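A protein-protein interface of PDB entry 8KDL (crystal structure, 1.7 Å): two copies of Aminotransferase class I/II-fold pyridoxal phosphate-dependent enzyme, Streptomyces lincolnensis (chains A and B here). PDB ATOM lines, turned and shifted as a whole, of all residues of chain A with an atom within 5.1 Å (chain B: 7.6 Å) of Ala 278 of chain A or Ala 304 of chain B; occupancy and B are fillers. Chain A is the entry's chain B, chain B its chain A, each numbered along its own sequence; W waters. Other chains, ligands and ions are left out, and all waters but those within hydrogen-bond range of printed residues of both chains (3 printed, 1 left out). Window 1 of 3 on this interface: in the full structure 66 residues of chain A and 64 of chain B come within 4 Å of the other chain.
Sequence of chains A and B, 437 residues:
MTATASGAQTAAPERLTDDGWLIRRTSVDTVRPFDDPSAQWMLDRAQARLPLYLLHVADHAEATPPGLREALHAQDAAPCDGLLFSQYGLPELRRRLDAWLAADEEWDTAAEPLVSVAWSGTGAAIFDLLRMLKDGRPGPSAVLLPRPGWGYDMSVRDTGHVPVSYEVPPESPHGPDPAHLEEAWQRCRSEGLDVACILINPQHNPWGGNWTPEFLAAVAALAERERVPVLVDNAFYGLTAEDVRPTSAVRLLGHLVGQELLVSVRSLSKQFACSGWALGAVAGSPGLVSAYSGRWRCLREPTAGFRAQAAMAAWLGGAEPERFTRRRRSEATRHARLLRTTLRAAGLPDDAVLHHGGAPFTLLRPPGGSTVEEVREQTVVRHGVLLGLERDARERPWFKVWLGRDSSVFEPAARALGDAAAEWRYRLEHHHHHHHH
Ala 278 of chain A touches just one residue of chain B: Ala 304 (3.9 Å). Ala 304 of chain B touches two residues of chain A. Of the printed residues of chain B, Gly 121 of chain A touches Pro 302. Printed residues of chain A within 4 Å of Pro 302 of chain B: Ser 120 and Gly 121. Of the printed residues of chain B, Ser 275 of chain A touches Asp 81 and Leu 83. Arg 307 of chain B touches none of the printed residues of chain A. The nearest printed residue of chain A that does not touch Asp 81 of chain B is Ser 269 of chain A (6.3 Å).
Among the printed residues, merely in contact across the chains: Ser 120 of chain A with Pro 302 of chain B, Cys 274 of chain A with Asp 81 of chain B, Gly 276 of chain A with Ala 304 of chain B, Ser 275 of chain A with Leu 83 of chain B, Ala 278 of chain A with Ala 304 of chain B and Gly 121 of chain A with Pro 302 of chain B.
4 positions are printed for both chains.
Water W1 lies within hydrogen-bond range of the side-chain carboxylate of Glu 301 of chain B (2.7 Å), the backbone carbonyl oxygen of Ser 120 of chain A (2.9 Å) and the indole nitrogen of Trp 119 of chain B (3.2 Å). Water W3 lies within hydrogen-bond range of the backbone carbonyl oxygen (O) of Ser 120 of chain B (2.9 Å) and the indole nitrogen (NE1) of Trp 119 of chain A (3.3 Å). Water W2 lies within hydrogen-bond range of N of Ser 275 of chain A (2.9 Å), N of Cys 274 of chain A (3.3 Å) and O of Asp 81 of chain B (3.4 Å).
Of the 22 printed residues of chain B, 5 touch a printed residue of chain A. Printed residues of chain B that touch a printed residue of chain A: Asp 81, Leu 83, Pro 302, Ala 304 and Gly 305. Hydrophobic or aromatic side chains of chain B within 4 Å of the printed part of chain A: Leu 83, Pro 302 and Ala 304. Hydrophobic or aromatic side chains of chain A within 4 Å of the printed part of chain B: Trp 277 and Ala 278. Among the printed residues, 10 pairs touch across the chains. Among the printed residues, no Asp or Glu carboxylate lies within 4 Å of a Lys or Arg side-chain nitrogen of the other chain.
NH2 of Arg 307 of chain B is in salt-bridge range of OD2 of Asp 81 of chain B. The indole nitrogen (NE1) of Trp 119 of chain B sits at hydrogen-bond distance from the backbone carbonyl oxygen (O) of Pro 302 of chain B, at 2.9 Å. The side-chain amide nitrogen of Gln 309 of chain B lies within hydrogen-bond range of the backbone carbonyl oxygen of Ala 304 of chain B (3.0 Å). The backbone NH (N) of Ser 120 of chain A is in hydrogen-bond range of the backbone carbonyl oxygen (O) of Ala 278 of chain A (3.3 Å). The backbone carbonyl oxygen of Ser 269 of chain A is in hydrogen-bond range of the backbone NH of Cys 274 of chain A, at 2.8 Å. N of Ser 275 of chain A sits at hydrogen-bond distance from O of Ser 269 of chain A (3.3 Å).
O of Asp 81 of chain B lies within hydrogen-bond range of N of Ser 275 of chain A, at 3.2 Å. The backbone carbonyl oxygen of Asp 81 of chain B lies within hydrogen-bond range of the backbone NH of Gly 276 of chain A. The side-chain carboxylate of Asp 81 of chain B is in hydrogen-bond range of the indole nitrogen of Trp 277 of chain A, at 2.8 Å. The backbone NH (N) of Gly 305 of chain B lies within hydrogen-bond range of the backbone carbonyl oxygen (O) of Gly 276 of chain A, at 2.9 Å.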
ATOM      1  N   ALA A 118       4.477 -11.697  -1.311  1.00  0.00           N
ATOM      2  CA  ALA A 118       4.039 -10.418  -1.875  1.00  0.00           C
ATOM      3  C   ALA A 118       3.191 -10.706  -3.110  1.00  0.00           C
ATOM      4  O   ALA A 118       3.563 -11.545  -3.940  1.00  0.00           O
ATOM      5  CB  ALA A 118       5.242  -9.524  -2.217  1.00  0.00           C
ATOM      6  N   TRP A 119       2.033 -10.025  -3.227  1.00  0.00           N
ATOM      7  CA  TRP A 119       1.101 -10.333  -4.312  1.00  0.00           C
ATOM      8  C   TRP A 119       0.683  -9.119  -5.139  1.00  0.00           C
ATOM      9  O   TRP A 119      -0.293  -9.200  -5.902  1.00  0.00           O
ATOM     10  CB  TRP A 119      -0.123 -11.054  -3.752  1.00  0.00           C
ATOM     11  CG  TRP A 119      -0.817 -10.297  -2.655  1.00  0.00           C
ATOM     12  CD1 TRP A 119      -1.669  -9.233  -2.793  1.00  0.00           C
ATOM     13  CD2 TRP A 119      -0.711 -10.550  -1.250  1.00  0.00           C
ATOM     14  NE1 TRP A 119      -2.098  -8.808  -1.552  1.00  0.00           N
ATOM     15  CE2 TRP A 119      -1.514  -9.594  -0.592  1.00  0.00           C
ATOM     16  CE3 TRP A 119      -0.005 -11.479  -0.479  1.00  0.00           C
ATOM     17  CZ2 TRP A 119      -1.652  -9.565   0.794  1.00  0.00           C
ATOM     18  CZ3 TRP A 119      -0.134 -11.436   0.892  1.00  0.00           C
ATOM     19  CH2 TRP A 119      -0.956 -10.491   1.519  1.00  0.00           C
ATOM     20  N   SER A 120       1.415  -8.007  -5.055  1.00  0.00           N
ATOM     21  CA  SER A 120       1.132  -6.881  -5.943  1.00  0.00           C
ATOM     22  C   SER A 120       2.401  -6.288  -6.555  1.00  0.00           C
ATOM     23  O   SER A 120       2.360  -5.174  -7.110  1.00  0.00           O
ATOM     24  CB  SER A 120       0.332  -5.806  -5.199  1.00  0.00           C
ATOM     25  OG  SER A 120       1.127  -5.213  -4.182  1.00  0.00           O
ATOM     26  N   GLY A 121       3.513  -7.005  -6.504  1.00  0.00           N
ATOM     27  CA  GLY A 121       4.771  -6.545  -7.080  1.00  0.00           C
ATOM     28  C   GLY A 121       5.847  -6.313  -6.031  1.00  0.00           C
ATOM     29  O   GLY A 121       5.579  -5.795  -4.938  1.00  0.00           O
ATOM     30  N   SER A 269       7.367 -13.748 -10.635  1.00  0.00           N
ATOM     31  CA  SER A 269       6.726 -13.541 -11.913  1.00  0.00           C
ATOM     32  C   SER A 269       7.716 -13.124 -13.010  1.00  0.00           C
ATOM     33  O   SER A 269       7.463 -13.305 -14.206  1.00  0.00           O
ATOM     34  CB  SER A 269       5.617 -12.517 -11.709  1.00  0.00           C
ATOM     35  OG  SER A 269       4.696 -13.016 -10.747  1.00  0.00           O
ATOM     36  N   CYS A 274       5.456 -14.703 -15.634  1.00  0.00           N
ATOM     37  CA  CYS A 274       4.057 -14.468 -15.292  1.00  0.00           C
ATOM     38  C   CYS A 274       3.932 -13.124 -14.588  1.00  0.00           C
ATOM     39  O   CYS A 274       3.325 -13.004 -13.519  1.00  0.00           O
ATOM     40  CB  CYS A 274       3.487 -15.594 -14.430  1.00  0.00           C
ATOM     41  SG  CYS A 274       4.420 -15.949 -12.956  1.00  0.00           S
ATOM     42  N   SER A 275       4.523 -12.097 -15.206  1.00  0.00           N
ATOM     43  CA  SER A 275       4.586 -10.777 -14.595  1.00  0.00           C
ATOM     44  C   SER A 275       3.215 -10.260 -14.218  1.00  0.00           C
ATOM     45  O   SER A 275       3.079  -9.590 -13.193  1.00  0.00           O
ATOM     46  CB  SER A 275       5.285  -9.777 -15.517  1.00  0.00           C
ATOM     47  OG  SER A 275       6.651 -10.090 -15.644  1.00  0.00           O
ATOM     48  N   GLY A 276       2.181 -10.604 -14.988  1.00  0.00           N
ATOM     49  CA  GLY A 276       0.831 -10.170 -14.649  1.00  0.00           C
ATOM     50  C   GLY A 276       0.328 -10.676 -13.306  1.00  0.00           C
ATOM     51  O   GLY A 276      -0.608 -10.095 -12.744  1.00  0.00           O
ATOM     52  N   TRP A 277       0.896 -11.772 -12.790  1.00  0.00           N
ATOM     53  CA  TRP A 277       0.423 -12.337 -11.535  1.00  0.00           C
ATOM     54  C   TRP A 277       1.025 -11.634 -10.322  1.00  0.00           C
ATOM     55  O   TRP A 277       0.525 -11.813  -9.203  1.00  0.00           O
ATOM     56  CB  TRP A 277       0.766 -13.825 -11.467  1.00  0.00           C
ATOM     57  CG  TRP A 277       0.132 -14.722 -12.505  1.00  0.00           C
ATOM     58  CD1 TRP A 277      -0.346 -14.375 -13.736  1.00  0.00           C
ATOM     59  CD2 TRP A 277      -0.037 -16.128 -12.387  1.00  0.00           C
ATOM     60  NE1 TRP A 277      -0.826 -15.491 -14.386  1.00  0.00           N
ATOM     61  CE2 TRP A 277      -0.635 -16.582 -13.580  1.00  0.00           C
ATOM     62  CE3 TRP A 277       0.262 -17.054 -11.377  1.00  0.00           C
ATOM     63  CZ2 TRP A 277      -0.949 -17.922 -13.796  1.00  0.00           C
ATOM     64  CZ3 TRP A 277      -0.046 -18.380 -11.588  1.00  0.00           C
ATOM     65  CH2 TRP A 277      -0.646 -18.808 -12.795  1.00  0.00           C
ATOM     66  N   ALA A 278       2.108 -10.890 -10.530  1.00  0.00           N
ATOM     67  CA  ALA A 278       2.749 -10.044  -9.519  1.00  0.00           C
ATOM     68  C   ALA A 278       2.983 -10.791  -8.201  1.00  0.00           C
ATOM     69  O   ALA A 278       2.682 -10.289  -7.120  1.00  0.00           O
ATOM     70  CB  ALA A 278       1.929  -8.775  -9.287  1.00  0.00           C
ATOM     71  N   LEU A 279       3.545 -11.997  -8.301  1.00  0.00           N
ATOM     72  CA  LEU A 279       3.861 -12.822  -7.138  1.00  0.00           C
ATOM     73  C   LEU A 279       5.342 -12.764  -6.800  1.00  0.00           C
ATOM     74  O   LEU A 279       6.201 -12.797  -7.689  1.00  0.00           O
ATOM     75  CB  LEU A 279       3.458 -14.280  -7.367  1.00  0.00           C
ATOM     76  CG  LEU A 279       1.966 -14.502  -7.572  1.00  0.00           C
ATOM     77  CD1 LEU A 279       1.653 -15.983  -7.726  1.00  0.00           C
ATOM     78  CD2 LEU A 279       1.227 -13.913  -6.376  1.00  0.00           C
ATOM     79  N   GLY A 280       5.632 -12.712  -5.505  1.00  0.00           N
ATOM     80  CA  GLY A 280       7.003 -12.601  -5.048  1.00  0.00           C
ATOM     81  C   GLY A 280       7.114 -13.050  -3.611  1.00  0.00           C
ATOM     82  O   GLY A 280       6.118 -13.357  -2.951  1.00  0.00           O
ATOM     83  N   ASP B  81      -0.264 -12.837 -19.868  1.00  0.00           N
ATOM     84  CA  ASP B  81       0.263 -12.816 -18.509  1.00  0.00           C
ATOM     85  C   ASP B  81       1.519 -11.970 -18.377  1.00  0.00           C
ATOM     86  O   ASP B  81       2.204 -12.049 -17.343  1.00  0.00           O
ATOM     87  CB  ASP B  81       0.513 -14.244 -18.019  1.00  0.00           C
ATOM     88  CG  ASP B  81      -0.773 -15.053 -17.919  1.00  0.00           C
ATOM     89  OD1 ASP B  81      -1.600 -14.776 -17.025  1.00  0.00           O
ATOM     90  OD2 ASP B  81      -0.985 -15.935 -18.776  1.00  0.00           O
ATOM     91  N   GLY B  82       1.823 -11.138 -19.374  1.00  0.00           N
ATOM     92  CA  GLY B  82       2.888 -10.159 -19.251  1.00  0.00           C
ATOM     93  C   GLY B  82       2.384  -8.830 -18.684  1.00  0.00           C
ATOM     94  O   GLY B  82       1.207  -8.646 -18.380  1.00  0.00           O
ATOM     95  N   LEU B  83       3.318  -7.894 -18.528  1.00  0.00           N
ATOM     96  CA  LEU B  83       2.963  -6.539 -18.126  1.00  0.00           C
ATOM     97  C   LEU B  83       2.307  -5.765 -19.273  1.00  0.00           C
ATOM     98  O   LEU B  83       2.622  -5.969 -20.442  1.00  0.00           O
ATOM     99  CB  LEU B  83       4.207  -5.786 -17.677  1.00  0.00           C
ATOM    100  CG  LEU B  83       4.957  -6.387 -16.484  1.00  0.00           C
ATOM    101  CD1 LEU B  83       6.256  -5.596 -16.266  1.00  0.00           C
ATOM    102  CD2 LEU B  83       4.100  -6.399 -15.239  1.00  0.00           C
ATOM    103  N   LEU B  84       1.420  -4.832 -18.912  1.00  0.00           N
ATOM    104  CA  LEU B  84       0.712  -3.991 -19.885  1.00  0.00           C
ATOM    105  C   LEU B  84       1.466  -2.702 -20.172  1.00  0.00           C
ATOM    106  O   LEU B  84       2.156  -2.152 -19.308  1.00  0.00           O
ATOM    107  CB  LEU B  84      -0.688  -3.604 -19.382  1.00  0.00           C
ATOM    108  CG  LEU B  84      -1.612  -4.643 -18.782  1.00  0.00           C
ATOM    109  CD1 LEU B  84      -2.987  -4.060 -18.443  1.00  0.00           C
ATOM    110  CD2 LEU B  84      -1.760  -5.762 -19.772  1.00  0.00           C
ATOM    111  N   SER B  86       0.168   0.341 -20.622  1.00  0.00           N
ATOM    112  CA  SER B  86      -0.707   1.474 -20.351  1.00  0.00           C
ATOM    113  C   SER B  86      -0.699   1.728 -18.853  1.00  0.00           C
ATOM    114  O   SER B  86      -0.701   0.783 -18.064  1.00  0.00           O
ATOM    115  CB  SER B  86      -2.146   1.233 -20.809  1.00  0.00           C
ATOM    116  OG  SER B  86      -2.940   2.362 -20.482  1.00  0.00           O
ATOM    117  N   GLY B  89      -4.461   0.647 -17.224  1.00  0.00           N
ATOM    118  CA  GLY B  89      -4.982  -0.704 -17.290  1.00  0.00           C
ATOM    119  C   GLY B  89      -5.264  -1.133 -18.719  1.00  0.00           C
ATOM    120  O   GLY B  89      -5.039  -0.406 -19.687  1.00  0.00           O
ATOM    121  N   LEU B  90      -5.744  -2.353 -18.839  1.00  0.00           N
ATOM    122  CA  LEU B  90      -6.018  -2.942 -20.148  1.00  0.00           C
ATOM    123  C   LEU B  90      -7.119  -2.168 -20.864  1.00  0.00           C
ATOM    124  O   LEU B  90      -8.225  -2.034 -20.318  1.00  0.00           O
ATOM    125  CB  LEU B  90      -6.424  -4.406 -19.951  1.00  0.00           C
ATOM    126  CG  LEU B  90      -6.540  -5.241 -21.227  1.00  0.00           C
ATOM    127  CD1 LEU B  90      -5.171  -5.376 -21.861  1.00  0.00           C
ATOM    128  CD2 LEU B  90      -7.099  -6.617 -20.862  1.00  0.00           C
ATOM    129  N   VAL B 117      -8.273   1.779 -14.540  1.00  0.00           N
ATOM    130  CA  VAL B 117      -8.404   0.513 -13.813  1.00  0.00           C
ATOM    131  C   VAL B 117      -7.490   0.548 -12.588  1.00  0.00           C
ATOM    132  O   VAL B 117      -6.331   0.969 -12.668  1.00  0.00           O
ATOM    133  CB  VAL B 117      -8.061  -0.693 -14.710  1.00  0.00           C
ATOM    134  CG1 VAL B 117      -8.224  -2.024 -13.937  1.00  0.00           C
ATOM    135  CG2 VAL B 117      -8.931  -0.703 -15.979  1.00  0.00           C
ATOM    136  N   ALA B 118      -8.014   0.090 -11.461  1.00  0.00           N
ATOM    137  CA  ALA B 118      -7.215  -0.279 -10.294  1.00  0.00           C
ATOM    138  C   ALA B 118      -7.161  -1.797 -10.216  1.00  0.00           C
ATOM    139  O   ALA B 118      -8.191  -2.465 -10.371  1.00  0.00           O
ATOM    140  CB  ALA B 118      -7.809   0.307  -9.009  1.00  0.00           C
ATOM    141  N   TRP B 119      -5.959  -2.345  -9.983  1.00  0.00           N
ATOM    142  CA  TRP B 119      -5.771  -3.793 -10.033  1.00  0.00           C
ATOM    143  C   TRP B 119      -5.114  -4.359  -8.776  1.00  0.00           C
ATOM    144  O   TRP B 119      -4.685  -5.520  -8.771  1.00  0.00           O
ATOM    145  CB  TRP B 119      -4.979  -4.165 -11.288  1.00  0.00           C
ATOM    146  CG  TRP B 119      -3.644  -3.462 -11.418  1.00  0.00           C
ATOM    147  CD1 TRP B 119      -2.471  -3.786 -10.781  1.00  0.00           C
ATOM    148  CD2 TRP B 119      -3.359  -2.318 -12.226  1.00  0.00           C
ATOM    149  NE1 TRP B 119      -1.477  -2.908 -11.155  1.00  0.00           N
ATOM    150  CE2 TRP B 119      -1.996  -2.002 -12.045  1.00  0.00           C
ATOM    151  CE3 TRP B 119      -4.117  -1.537 -13.104  1.00  0.00           C
ATOM    152  CZ2 TRP B 119      -1.381  -0.931 -12.707  1.00  0.00           C
ATOM    153  CZ3 TRP B 119      -3.507  -0.473 -13.753  1.00  0.00           C
ATOM    154  CH2 TRP B 119      -2.150  -0.186 -13.558  1.00  0.00           C
ATOM    155  N   SER B 120      -5.070  -3.603  -7.686  1.00  0.00           N
ATOM    156  CA  SER B 120      -4.505  -4.175  -6.467  1.00  0.00           C
ATOM    157  C   SER B 120      -5.358  -3.849  -5.243  1.00  0.00           C
ATOM    158  O   SER B 120      -4.889  -4.017  -4.103  1.00  0.00           O
ATOM    159  CB  SER B 120      -3.063  -3.684  -6.249  1.00  0.00           C
ATOM    160  OG  SER B 120      -3.040  -2.287  -5.989  1.00  0.00           O
ATOM    161  N   LEU B 279      -9.872  -6.098  -8.689  1.00  0.00           N
ATOM    162  CA  LEU B 279     -10.140  -5.183  -9.794  1.00  0.00           C
ATOM    163  C   LEU B 279     -11.157  -4.125  -9.390  1.00  0.00           C
ATOM    164  O   LEU B 279     -12.132  -4.413  -8.685  1.00  0.00           O
ATOM    165  CB  LEU B 279     -10.663  -5.929 -11.025  1.00  0.00           C
ATOM    166  CG  LEU B 279      -9.733  -7.003 -11.587  1.00  0.00           C
ATOM    167  CD1 LEU B 279     -10.323  -7.589 -12.861  1.00  0.00           C
ATOM    168  CD2 LEU B 279      -8.354  -6.398 -11.865  1.00  0.00           C
ATOM    169  N   CYS B 298       1.697   3.859 -10.972  1.00  0.00           N
ATOM    170  CA  CYS B 298       2.534   2.982 -11.790  1.00  0.00           C
ATOM    171  C   CYS B 298       4.024   3.106 -11.489  1.00  0.00           C
ATOM    172  O   CYS B 298       4.796   2.232 -11.898  1.00  0.00           O
ATOM    173  CB  CYS B 298       2.288   3.241 -13.277  1.00  0.00           C
ATOM    174  SG  CYS B 298       0.822   2.365 -13.885  1.00  0.00           S
ATOM    175  N   GLU B 301       3.676   0.337  -8.444  1.00  0.00           N
ATOM    176  CA  GLU B 301       3.107  -0.956  -8.814  1.00  0.00           C
ATOM    177  C   GLU B 301       3.442  -1.298 -10.253  1.00  0.00           C
ATOM    178  O   GLU B 301       3.491  -0.411 -11.113  1.00  0.00           O
ATOM    179  CB  GLU B 301       1.576  -0.949  -8.699  1.00  0.00           C
ATOM    180  CG  GLU B 301       1.041  -0.761  -7.317  1.00  0.00           C
ATOM    181  CD  GLU B 301      -0.381  -1.273  -7.170  1.00  0.00           C
ATOM    182  OE1 GLU B 301      -0.842  -1.995  -8.060  1.00  0.00           O
ATOM    183  OE2 GLU B 301      -1.045  -0.938  -6.165  1.00  0.00           O
ATOM    184  N   PRO B 302       3.631  -2.573 -10.561  1.00  0.00           N
ATOM    185  CA  PRO B 302       3.708  -2.987 -11.967  1.00  0.00           C
ATOM    186  C   PRO B 302       2.330  -2.936 -12.599  1.00  0.00           C
ATOM    187  O   PRO B 302       1.313  -2.935 -11.907  1.00  0.00           O
ATOM    188  CB  PRO B 302       4.217  -4.425 -11.880  1.00  0.00           C
ATOM    189  CG  PRO B 302       3.633  -4.919 -10.580  1.00  0.00           C
ATOM    190  CD  PRO B 302       3.648  -3.726  -9.642  1.00  0.00           C
ATOM    191  N   THR B 303       2.314  -2.866 -13.936  1.00  0.00           N
ATOM    192  CA  THR B 303       1.068  -2.909 -14.713  1.00  0.00           C
ATOM    193  C   THR B 303       0.605  -4.364 -14.830  1.00  0.00           C
ATOM    194  O   THR B 303       0.643  -4.989 -15.892  1.00  0.00           O
ATOM    195  CB  THR B 303       1.264  -2.262 -16.076  1.00  0.00           C
ATOM    196  OG1 THR B 303       2.465  -2.748 -16.687  1.00  0.00           O
ATOM    197  CG2 THR B 303       1.394  -0.734 -15.914  1.00  0.00           C
ATOM    198  N   ALA B 304       0.162  -4.899 -13.689  1.00  0.00           N
ATOM    199  CA  ALA B 304      -0.169  -6.304 -13.496  1.00  0.00           C
ATOM    200  C   ALA B 304      -1.624  -6.576 -13.870  1.00  0.00           C
ATOM    201  O   ALA B 304      -2.375  -5.677 -14.260  1.00  0.00           O
ATOM    202  CB  ALA B 304       0.106  -6.704 -12.040  1.00  0.00           C
ATOM    203  N   GLY B 305      -2.038  -7.837 -13.740  1.00  0.00           N
ATOM    204  CA  GLY B 305      -3.437  -8.188 -13.893  1.00  0.00           C
ATOM    205  C   GLY B 305      -3.948  -8.368 -15.308  1.00  0.00           C
ATOM    206  O   GLY B 305      -5.165  -8.382 -15.502  1.00  0.00           O
ATOM    207  N   PHE B 306      -3.061  -8.528 -16.294  1.00  0.00           N
ATOM    208  CA  PHE B 306      -3.476  -8.632 -17.698  1.00  0.00           C
ATOM    209  C   PHE B 306      -4.612  -9.653 -17.863  1.00  0.00           C
ATOM    210  O   PHE B 306      -5.707  -9.319 -18.344  1.00  0.00           O
ATOM    211  CB  PHE B 306      -2.224  -8.973 -18.539  1.00  0.00           C
ATOM    212  CG  PHE B 306      -2.393  -8.940 -20.057  1.00  0.00           C
ATOM    213  CD1 PHE B 306      -3.633  -8.835 -20.688  1.00  0.00           C
ATOM    214  CD2 PHE B 306      -1.248  -8.973 -20.859  1.00  0.00           C
ATOM    215  CE1 PHE B 306      -3.712  -8.816 -22.103  1.00  0.00           C
ATOM    216  CE2 PHE B 306      -1.315  -8.951 -22.251  1.00  0.00           C
ATOM    217  CZ  PHE B 306      -2.559  -8.868 -22.876  1.00  0.00           C
ATOM    218  N   ARG B 307      -4.389 -10.896 -17.426  1.00  0.00           N
ATOM    219  CA  ARG B 307      -5.384 -11.941 -17.677  1.00  0.00           C
ATOM    220  C   ARG B 307      -6.690 -11.670 -16.931  1.00  0.00           C
ATOM    221  O   ARG B 307      -7.787 -11.848 -17.481  1.00  0.00           O
ATOM    222  CB  ARG B 307      -4.832 -13.306 -17.267  1.00  0.00           C
ATOM    223  CG  ARG B 307      -5.875 -14.428 -17.413  1.00  0.00           C
ATOM    224  CD  ARG B 307      -5.304 -15.746 -16.864  1.00  0.00           C
ATOM    225  NE  ARG B 307      -4.196 -16.183 -17.703  1.00  0.00           N
ATOM    226  CZ  ARG B 307      -4.316 -16.981 -18.759  1.00  0.00           C
ATOM    227  NH1 ARG B 307      -5.499 -17.451 -19.143  1.00  0.00           N
ATOM    228  NH2 ARG B 307      -3.226 -17.318 -19.445  1.00  0.00           N
ATOM    229  N   ALA B 308      -6.597 -11.235 -15.678  1.00  0.00           N
ATOM    230  CA  ALA B 308      -7.810 -10.973 -14.911  1.00  0.00           C
ATOM    231  C   ALA B 308      -8.615  -9.832 -15.531  1.00  0.00           C
ATOM    232  O   ALA B 308      -9.852  -9.898 -15.629  1.00  0.00           O
ATOM    233  CB  ALA B 308      -7.432 -10.659 -13.458  1.00  0.00           C
ATOM    234  N   GLN B 309      -7.925  -8.784 -15.970  1.00  0.00           N
ATOM    235  CA  GLN B 309      -8.606  -7.652 -16.591  1.00  0.00           C
ATOM    236  C   GLN B 309      -9.285  -8.074 -17.885  1.00  0.00           C
ATOM    237  O   GLN B 309     -10.401  -7.617 -18.189  1.00  0.00           O
ATOM    238  CB  GLN B 309      -7.598  -6.538 -16.864  1.00  0.00           C
ATOM    239  CG  GLN B 309      -7.057  -5.888 -15.593  1.00  0.00           C
ATOM    240  CD  GLN B 309      -6.208  -4.669 -15.875  1.00  0.00           C
ATOM    241  OE1 GLN B 309      -6.635  -3.756 -16.574  1.00  0.00           O
ATOM    242  NE2 GLN B 309      -4.972  -4.665 -15.346  1.00  0.00           N
HETATM  243  O   HOH W   1       0.050  -4.430  -8.777  1.00  0.00           O
HETATM  244  O   HOH W   2       5.560 -12.297 -17.926  1.00  0.00           O
HETATM  245  O   HOH W   3      -3.302  -6.391  -3.516  1.00  0.00           O
